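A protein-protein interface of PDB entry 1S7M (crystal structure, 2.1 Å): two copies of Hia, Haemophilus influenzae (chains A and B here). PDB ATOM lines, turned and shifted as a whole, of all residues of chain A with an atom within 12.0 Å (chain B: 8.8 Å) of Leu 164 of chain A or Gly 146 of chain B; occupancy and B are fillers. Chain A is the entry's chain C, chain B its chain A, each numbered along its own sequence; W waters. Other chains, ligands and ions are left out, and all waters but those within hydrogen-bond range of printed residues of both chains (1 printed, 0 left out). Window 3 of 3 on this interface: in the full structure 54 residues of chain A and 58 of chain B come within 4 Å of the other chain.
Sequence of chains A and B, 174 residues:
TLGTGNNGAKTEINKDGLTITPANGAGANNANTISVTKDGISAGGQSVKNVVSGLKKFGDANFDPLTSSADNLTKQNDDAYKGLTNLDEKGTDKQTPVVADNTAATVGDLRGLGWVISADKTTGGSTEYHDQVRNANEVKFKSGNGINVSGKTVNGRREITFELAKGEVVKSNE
Printed residues of chain B within 4 Å of Ile 147 of chain A: Ile 147.
Printed residues of chain B within 4 Å of Phe 162 of chain A: Ser 143, Gly 144, Ile 147 and Phe 162.
Of the printed residues of chain B, Glu 163 of chain A touches Asn 145 and Ile 147.
Of chain B, only Asn 145, Gly 146 and Ile 147 come within 4 Å of Leu 164 of chain A.
Lys 166 of chain A touches none of the printed residues of chain B.
Of the printed residues of chain A, Ser 143 of chain B touches Phe 162.
Gly 144 of chain B touches one residue of chain A.
Asn 145 of chain B touches just these residues of chain A: Glu 163 and Leu 164.
Of chain A, only Leu 164 (3.7 Å) comes within 4 Å of Gly 146 of chain B.
Of chain A, only Ile 147 (3.6 Å), Phe 162 (3.7 Å), Glu 163 (3.5 Å) and Leu 164 (3.97 Å) come within 4 Å of Ile 147 of chain B.
Asn 148 of chain B touches none of the printed residues of chain A.
Of the printed residues of chain A, Phe 162 of chain B touches Phe 162.
No residue of chain A comes within 4 Å of Leu 164 of chain B.
No residue of chain A comes within 4 Å of Ala 165 of chain B.
The nearest residue of chain A that does not touch Gly 146 of chain B is Glu 163 of chain A (5.6 Å).
Phe 162 of chain A touches Ile 147 of chain B, but with the chains exchanged Ile 147 of chain A does not touch Phe 162 of chain B (6.8 Å).
Phe 162 of chain B touches its own counterpart, Phe 162 of chain A.
Glu 163 of chain A touches Asn 145 of chain B, but with the chains exchanged Asn 145 of chain A does not touch Glu 163 of chain B (11.9 Å).
Glu 163 of chain A touches Ile 147 of chain B, but with the chains exchanged Ile 147 of chain A does not touch Glu 163 of chain B (7.8 Å).
11 positions are printed for both chains.
Of the 16 printed residues of chain A, 4 touch a printed residue of chain B.
Among the printed residues, 10 pairs touch across the chains.
Among the printed residues, no Asp or Glu carboxylate lies within 4 Å of a Lys or Arg side-chain nitrogen of the other chain.
CG2 of Ile 147 of chain A touches CD1 of Ile 147 of chain B, at 3.6 Å.
Phe 162 of chain A touches Ser 143 of chain B (O to C, 3.8 Å).
Phe 162 of chain A touches Ile 147 of chain B (O to CB, 3.7 Å).
Phe 162 of chain A touches Phe 162 of chain B.
CA of Glu 163 of chain A touches O of Asn 145 of chain B, 3.6 Å away.
Ile 147 of chain B touches Glu 163 of chain A (CD1 to C, 3.5 Å).
Leu 164 of chain A touches Gly 146 of chain B (CD1 to CA, 3.7 Å).
N of Leu 164 of chain A touches CD1 of Ile 147 of chain B (3.97 Å).
Water W1 bridges the side-chain carboxylate of Glu 163 of chain A (2.8 Å) and the backbone NH of Asn 145 of chain B (3.3 Å).
The backbone NH (N) of Val 149 of chain B sits at hydrogen-bond distance from the side-chain hydroxyl (OG) of Ser 143 of chain B (2.5 Å).
The backbone NH of Ala 165 of chain B lies within hydrogen-bond range of the backbone carbonyl oxygen of Gly 146 of chain B.
The backbone NH (N) of Asn 148 of chain A lies within hydrogen-bond range of the backbone carbonyl oxygen (O) of Glu 163 of chain A (2.9 Å).
The backbone NH (N) of Gly 144 of chain B is in hydrogen-bond range of the backbone carbonyl oxygen (O) of Phe 162 of chain A.
The backbone carbonyl oxygen of Asn 145 of chain B lies within hydrogen-bond range of the backbone NH of Leu 164 of chain A.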
ATOM      1  N   LYS A 142     -25.107   7.130   8.202  1.00  0.00           N
ATOM      2  CA  LYS A 142     -25.385   7.127   6.763  1.00  0.00           C
ATOM      3  C   LYS A 142     -24.253   6.810   5.818  1.00  0.00           C
ATOM      4  O   LYS A 142     -23.134   7.288   5.990  1.00  0.00           O
ATOM      5  CB  LYS A 142     -25.934   8.494   6.334  1.00  0.00           C
ATOM      6  CG  LYS A 142     -27.177   8.974   7.071  1.00  0.00           C
ATOM      7  CD  LYS A 142     -28.451   8.408   6.469  1.00  0.00           C
ATOM      8  CE  LYS A 142     -28.682   8.923   5.051  1.00  0.00           C
ATOM      9  NZ  LYS A 142     -28.471  10.399   4.980  1.00  0.00           N
ATOM     10  N   SER A 143     -24.567   6.028   4.792  1.00  0.00           N
ATOM     11  CA  SER A 143     -23.588   5.685   3.771  1.00  0.00           C
ATOM     12  C   SER A 143     -23.362   6.960   2.987  1.00  0.00           C
ATOM     13  O   SER A 143     -24.175   7.866   3.013  1.00  0.00           O
ATOM     14  CB  SER A 143     -24.121   4.599   2.835  1.00  0.00           C
ATOM     15  OG  SER A 143     -24.305   3.371   3.519  1.00  0.00           O
ATOM     16  N   GLY A 144     -22.240   7.046   2.307  1.00  0.00           N
ATOM     17  CA  GLY A 144     -21.960   8.234   1.536  1.00  0.00           C
ATOM     18  C   GLY A 144     -21.168   7.767   0.339  1.00  0.00           C
ATOM     19  O   GLY A 144     -20.984   6.558   0.150  1.00  0.00           O
ATOM     20  N   ASN A 145     -20.680   8.719  -0.447  1.00  0.00           N
ATOM     21  CA  ASN A 145     -19.922   8.404  -1.639  1.00  0.00           C
ATOM     22  C   ASN A 145     -18.724   7.492  -1.403  1.00  0.00           C
ATOM     23  O   ASN A 145     -17.741   7.885  -0.769  1.00  0.00           O
ATOM     24  CB  ASN A 145     -19.453   9.689  -2.317  1.00  0.00           C
ATOM     25  CG  ASN A 145     -18.781   9.420  -3.638  1.00  0.00           C
ATOM     26  OD1 ASN A 145     -17.581   9.661  -3.801  1.00  0.00           O
ATOM     27  ND2 ASN A 145     -19.544   8.886  -4.589  1.00  0.00           N
ATOM     28  N   GLY A 146     -18.819   6.270  -1.912  1.00  0.00           N
ATOM     29  CA  GLY A 146     -17.734   5.322  -1.776  1.00  0.00           C
ATOM     30  C   GLY A 146     -17.653   4.534  -0.488  1.00  0.00           C
ATOM     31  O   GLY A 146     -16.714   3.743  -0.314  1.00  0.00           O
ATOM     32  N   ILE A 147     -18.616   4.734   0.413  1.00  0.00           N
ATOM     33  CA  ILE A 147     -18.623   4.021   1.687  1.00  0.00           C
ATOM     34  C   ILE A 147     -20.000   3.489   2.037  1.00  0.00           C
ATOM     35  O   ILE A 147     -20.978   4.241   2.058  1.00  0.00           O
ATOM     36  CB  ILE A 147     -18.143   4.928   2.864  1.00  0.00           C
ATOM     37  CG1 ILE A 147     -16.735   5.448   2.577  1.00  0.00           C
ATOM     38  CG2 ILE A 147     -18.126   4.131   4.174  1.00  0.00           C
ATOM     39  CD1 ILE A 147     -16.203   6.397   3.589  1.00  0.00           C
ATOM     40  N   ASN A 148     -20.071   2.186   2.292  1.00  0.00           N
ATOM     41  CA  ASN A 148     -21.318   1.547   2.684  1.00  0.00           C
ATOM     42  C   ASN A 148     -21.334   1.380   4.209  1.00  0.00           C
ATOM     43  O   ASN A 148     -20.441   0.747   4.772  1.00  0.00           O
ATOM     44  CB  ASN A 148     -21.444   0.171   2.024  1.00  0.00           C
ATOM     45  CG  ASN A 148     -21.753   0.260   0.533  1.00  0.00           C
ATOM     46  OD1 ASN A 148     -21.668  -0.739  -0.186  1.00  0.00           O
ATOM     47  ND2 ASN A 148     -22.121   1.451   0.066  1.00  0.00           N
ATOM     48  N   VAL A 149     -22.341   1.947   4.871  1.00  0.00           N
ATOM     49  CA  VAL A 149     -22.469   1.842   6.328  1.00  0.00           C
ATOM     50  C   VAL A 149     -23.703   0.989   6.639  1.00  0.00           C
ATOM     51  O   VAL A 149     -24.819   1.356   6.288  1.00  0.00           O
ATOM     52  CB  VAL A 149     -22.629   3.241   6.969  1.00  0.00           C
ATOM     53  CG1 VAL A 149     -22.658   3.131   8.490  1.00  0.00           C
ATOM     54  CG2 VAL A 149     -21.492   4.147   6.526  1.00  0.00           C
ATOM     55  N   SER A 150     -23.505  -0.153   7.286  1.00  0.00           N
ATOM     56  CA  SER A 150     -24.625  -1.033   7.612  1.00  0.00           C
ATOM     57  C   SER A 150     -24.673  -1.425   9.086  1.00  0.00           C
ATOM     58  O   SER A 150     -23.678  -1.326   9.810  1.00  0.00           O
ATOM     59  CB  SER A 150     -24.586  -2.297   6.749  1.00  0.00           C
ATOM     60  OG  SER A 150     -23.344  -2.968   6.865  1.00  0.00           O
ATOM     61  N   ILE A 160     -22.276  -1.529  13.882  1.00  0.00           N
ATOM     62  CA  ILE A 160     -22.347  -0.729  12.664  1.00  0.00           C
ATOM     63  C   ILE A 160     -21.036  -1.028  11.934  1.00  0.00           C
ATOM     64  O   ILE A 160     -19.944  -0.790  12.478  1.00  0.00           O
ATOM     65  CB  ILE A 160     -22.403   0.804  12.928  1.00  0.00           C
ATOM     66  CG1 ILE A 160     -23.568   1.168  13.859  1.00  0.00           C
ATOM     67  CG2 ILE A 160     -22.540   1.519  11.612  1.00  0.00           C
ATOM     68  CD1 ILE A 160     -24.933   0.514  13.496  1.00  0.00           C
ATOM     69  N   THR A 161     -21.137  -1.534  10.710  1.00  0.00           N
ATOM     70  CA  THR A 161     -19.963  -1.887   9.932  1.00  0.00           C
ATOM     71  C   THR A 161     -19.699  -0.896   8.827  1.00  0.00           C
ATOM     72  O   THR A 161     -20.627  -0.407   8.197  1.00  0.00           O
ATOM     73  CB  THR A 161     -20.132  -3.282   9.339  1.00  0.00           C
ATOM     74  OG1 THR A 161     -20.345  -4.204  10.407  1.00  0.00           O
ATOM     75  CG2 THR A 161     -18.897  -3.690   8.522  1.00  0.00           C
ATOM     76  N   PHE A 162     -18.418  -0.619   8.594  1.00  0.00           N
ATOM     77  CA  PHE A 162     -17.992   0.342   7.598  1.00  0.00           C
ATOM     78  C   PHE A 162     -17.079  -0.291   6.535  1.00  0.00           C
ATOM     79  O   PHE A 162     -16.012  -0.819   6.860  1.00  0.00           O
ATOM     80  CB  PHE A 162     -17.266   1.490   8.302  1.00  0.00           C
ATOM     81  CG  PHE A 162     -18.104   2.186   9.355  1.00  0.00           C
ATOM     82  CD1 PHE A 162     -18.360   1.579  10.578  1.00  0.00           C
ATOM     83  CD2 PHE A 162     -18.658   3.445   9.103  1.00  0.00           C
ATOM     84  CE1 PHE A 162     -19.155   2.209  11.544  1.00  0.00           C
ATOM     85  CE2 PHE A 162     -19.447   4.076  10.048  1.00  0.00           C
ATOM     86  CZ  PHE A 162     -19.697   3.456  11.275  1.00  0.00           C
ATOM     87  N   GLU A 163     -17.489  -0.235   5.270  1.00  0.00           N
ATOM     88  CA  GLU A 163     -16.683  -0.828   4.212  1.00  0.00           C
ATOM     89  C   GLU A 163     -16.675  -0.011   2.945  1.00  0.00           C
ATOM     90  O   GLU A 163     -17.489   0.896   2.763  1.00  0.00           O
ATOM     91  CB  GLU A 163     -17.189  -2.228   3.893  1.00  0.00           C
ATOM     92  CG  GLU A 163     -18.626  -2.239   3.458  1.00  0.00           C
ATOM     93  CD  GLU A 163     -19.137  -3.637   3.197  1.00  0.00           C
ATOM     94  OE1 GLU A 163     -18.732  -4.563   3.933  1.00  0.00           O
ATOM     95  OE2 GLU A 163     -19.957  -3.801   2.262  1.00  0.00           O
ATOM     96  N   LEU A 164     -15.733  -0.326   2.062  1.00  0.00           N
ATOM     97  CA  LEU A 164     -15.644   0.382   0.797  1.00  0.00           C
ATOM     98  C   LEU A 164     -16.765  -0.106  -0.114  1.00  0.00           C
ATOM     99  O   LEU A 164     -17.025  -1.304  -0.203  1.00  0.00           O
ATOM    100  CB  LEU A 164     -14.276   0.146   0.141  1.00  0.00           C
ATOM    101  CG  LEU A 164     -13.116   0.915   0.784  1.00  0.00           C
ATOM    102  CD1 LEU A 164     -11.809   0.538   0.105  1.00  0.00           C
ATOM    103  CD2 LEU A 164     -13.366   2.413   0.664  1.00  0.00           C
ATOM    104  N   ALA A 165     -17.444   0.831  -0.763  1.00  0.00           N
ATOM    105  CA  ALA A 165     -18.541   0.500  -1.669  1.00  0.00           C
ATOM    106  C   ALA A 165     -18.014   0.290  -3.086  1.00  0.00           C
ATOM    107  O   ALA A 165     -16.902   0.712  -3.414  1.00  0.00           O
ATOM    108  CB  ALA A 165     -19.580   1.614  -1.664  1.00  0.00           C
ATOM    109  N   LYS A 166     -18.836  -0.352  -3.914  1.00  0.00           N
ATOM    110  CA  LYS A 166     -18.526  -0.652  -5.315  1.00  0.00           C
ATOM    111  C   LYS A 166     -17.336  -1.591  -5.430  1.00  0.00           C
ATOM    112  O   LYS A 166     -16.602  -1.741  -4.427  1.00  0.00           O
ATOM    113  CB  LYS A 166     -18.255   0.641  -6.102  1.00  0.00           C
ATOM    114  N   SER B 143     -14.514  -2.249  11.763  1.00  0.00           N
ATOM    115  CA  SER B 143     -13.783  -2.005  10.541  1.00  0.00           C
ATOM    116  C   SER B 143     -14.369  -2.965   9.514  1.00  0.00           C
ATOM    117  O   SER B 143     -14.837  -4.052   9.852  1.00  0.00           O
ATOM    118  CB  SER B 143     -12.295  -2.310  10.747  1.00  0.00           C
ATOM    119  OG  SER B 143     -11.722  -1.415  11.683  1.00  0.00           O
ATOM    120  N   GLY B 144     -14.357  -2.552   8.262  1.00  0.00           N
ATOM    121  CA  GLY B 144     -14.876  -3.397   7.206  1.00  0.00           C
ATOM    122  C   GLY B 144     -13.836  -3.329   6.111  1.00  0.00           C
ATOM    123  O   GLY B 144     -12.866  -2.571   6.231  1.00  0.00           O
ATOM    124  N   ASN B 145     -14.030  -4.092   5.041  1.00  0.00           N
ATOM    125  CA  ASN B 145     -13.046  -4.097   3.978  1.00  0.00           C
ATOM    126  C   ASN B 145     -12.633  -2.709   3.499  1.00  0.00           C
ATOM    127  O   ASN B 145     -13.455  -1.918   3.025  1.00  0.00           O
ATOM    128  CB  ASN B 145     -13.521  -4.929   2.784  1.00  0.00           C
ATOM    129  CG  ASN B 145     -12.475  -4.986   1.682  1.00  0.00           C
ATOM    130  OD1 ASN B 145     -12.642  -4.395   0.615  1.00  0.00           O
ATOM    131  ND2 ASN B 145     -11.371  -5.678   1.954  1.00  0.00           N
ATOM    132  N   GLY B 146     -11.342  -2.431   3.644  1.00  0.00           N
ATOM    133  CA  GLY B 146     -10.778  -1.171   3.220  1.00  0.00           C
ATOM    134  C   GLY B 146     -10.890  -0.029   4.195  1.00  0.00           C
ATOM    135  O   GLY B 146     -10.350   1.045   3.933  1.00  0.00           O
ATOM    136  N   ILE B 147     -11.588  -0.225   5.314  1.00  0.00           N
ATOM    137  CA  ILE B 147     -11.737   0.865   6.277  1.00  0.00           C
ATOM    138  C   ILE B 147     -11.372   0.426   7.685  1.00  0.00           C
ATOM    139  O   ILE B 147     -11.800  -0.628   8.142  1.00  0.00           O
ATOM    140  CB  ILE B 147     -13.176   1.403   6.273  1.00  0.00           C
ATOM    141  CG1 ILE B 147     -13.550   1.869   4.859  1.00  0.00           C
ATOM    142  CG2 ILE B 147     -13.306   2.549   7.258  1.00  0.00           C
ATOM    143  CD1 ILE B 147     -14.956   2.484   4.753  1.00  0.00           C
ATOM    144  N   ASN B 148     -10.546   1.217   8.361  1.00  0.00           N
ATOM    145  CA  ASN B 148     -10.162   0.866   9.722  1.00  0.00           C
ATOM    146  C   ASN B 148     -10.869   1.758  10.722  1.00  0.00           C
ATOM    147  O   ASN B 148     -10.749   2.975  10.678  1.00  0.00           O
ATOM    148  CB  ASN B 148      -8.643   0.947   9.920  1.00  0.00           C
ATOM    149  CG  ASN B 148      -7.912  -0.254   9.323  1.00  0.00           C
ATOM    150  OD1 ASN B 148      -8.465  -1.366   9.242  1.00  0.00           O
ATOM    151  ND2 ASN B 148      -6.655  -0.041   8.914  1.00  0.00           N
ATOM    152  N   VAL B 149     -11.612   1.128  11.620  1.00  0.00           N
ATOM    153  CA  VAL B 149     -12.381   1.860  12.620  1.00  0.00           C
ATOM    154  C   VAL B 149     -11.793   1.658  14.018  1.00  0.00           C
ATOM    155  O   VAL B 149     -11.791   0.542  14.540  1.00  0.00           O
ATOM    156  CB  VAL B 149     -13.865   1.391  12.604  1.00  0.00           C
ATOM    157  CG1 VAL B 149     -14.697   2.284  13.476  1.00  0.00           C
ATOM    158  CG2 VAL B 149     -14.385   1.377  11.177  1.00  0.00           C
ATOM    159  N   PHE B 162     -12.144   7.118  11.762  1.00  0.00           N
ATOM    160  CA  PHE B 162     -12.323   6.371  10.517  1.00  0.00           C
ATOM    161  C   PHE B 162     -11.251   6.676   9.468  1.00  0.00           C
ATOM    162  O   PHE B 162     -11.091   7.818   9.054  1.00  0.00           O
ATOM    163  CB  PHE B 162     -13.712   6.680   9.930  1.00  0.00           C
ATOM    164  CG  PHE B 162     -14.846   6.366  10.864  1.00  0.00           C
ATOM    165  CD1 PHE B 162     -15.147   7.215  11.925  1.00  0.00           C
ATOM    166  CD2 PHE B 162     -15.576   5.189  10.713  1.00  0.00           C
ATOM    167  CE1 PHE B 162     -16.167   6.893  12.832  1.00  0.00           C
ATOM    168  CE2 PHE B 162     -16.600   4.847  11.612  1.00  0.00           C
ATOM    169  CZ  PHE B 162     -16.898   5.701  12.676  1.00  0.00           C
ATOM    170  N   GLU B 163     -10.538   5.648   9.021  1.00  0.00           N
ATOM    171  CA  GLU B 163      -9.501   5.854   8.016  1.00  0.00           C
ATOM    172  C   GLU B 163      -9.403   4.694   7.031  1.00  0.00           C
ATOM    173  O   GLU B 163      -9.783   3.559   7.340  1.00  0.00           O
ATOM    174  CB  GLU B 163      -8.140   6.027   8.705  1.00  0.00           C
ATOM    175  CG  GLU B 163      -7.750   4.790   9.508  1.00  0.00           C
ATOM    176  CD  GLU B 163      -6.415   4.925  10.232  1.00  0.00           C
ATOM    177  OE1 GLU B 163      -6.155   6.003  10.820  1.00  0.00           O
ATOM    178  OE2 GLU B 163      -5.638   3.937  10.224  1.00  0.00           O
ATOM    179  N   LEU B 164      -8.874   4.984   5.844  1.00  0.00           N
ATOM    180  CA  LEU B 164      -8.680   3.956   4.824  1.00  0.00           C
ATOM    181  C   LEU B 164      -7.647   2.988   5.369  1.00  0.00           C
ATOM    182  O   LEU B 164      -6.718   3.404   6.051  1.00  0.00           O
ATOM    183  CB  LEU B 164      -8.140   4.579   3.538  1.00  0.00           C
ATOM    184  CG  LEU B 164      -9.056   5.578   2.826  1.00  0.00           C
ATOM    185  CD1 LEU B 164      -8.288   6.287   1.705  1.00  0.00           C
ATOM    186  CD2 LEU B 164     -10.270   4.843   2.275  1.00  0.00           C
ATOM    187  N   ALA B 165      -7.808   1.703   5.081  1.00  0.00           N
ATOM    188  CA  ALA B 165      -6.852   0.702   5.542  1.00  0.00           C
ATOM    189  C   ALA B 165      -5.626   0.713   4.621  1.00  0.00           C
ATOM    190  O   ALA B 165      -5.584   1.573   3.710  1.00  0.00           O
ATOM    191  CB  ALA B 165      -7.490  -0.681   5.539  1.00  0.00           C
HETATM  192  O   HOH W   1     -16.685  -5.976   5.159  1.00  0.00           O
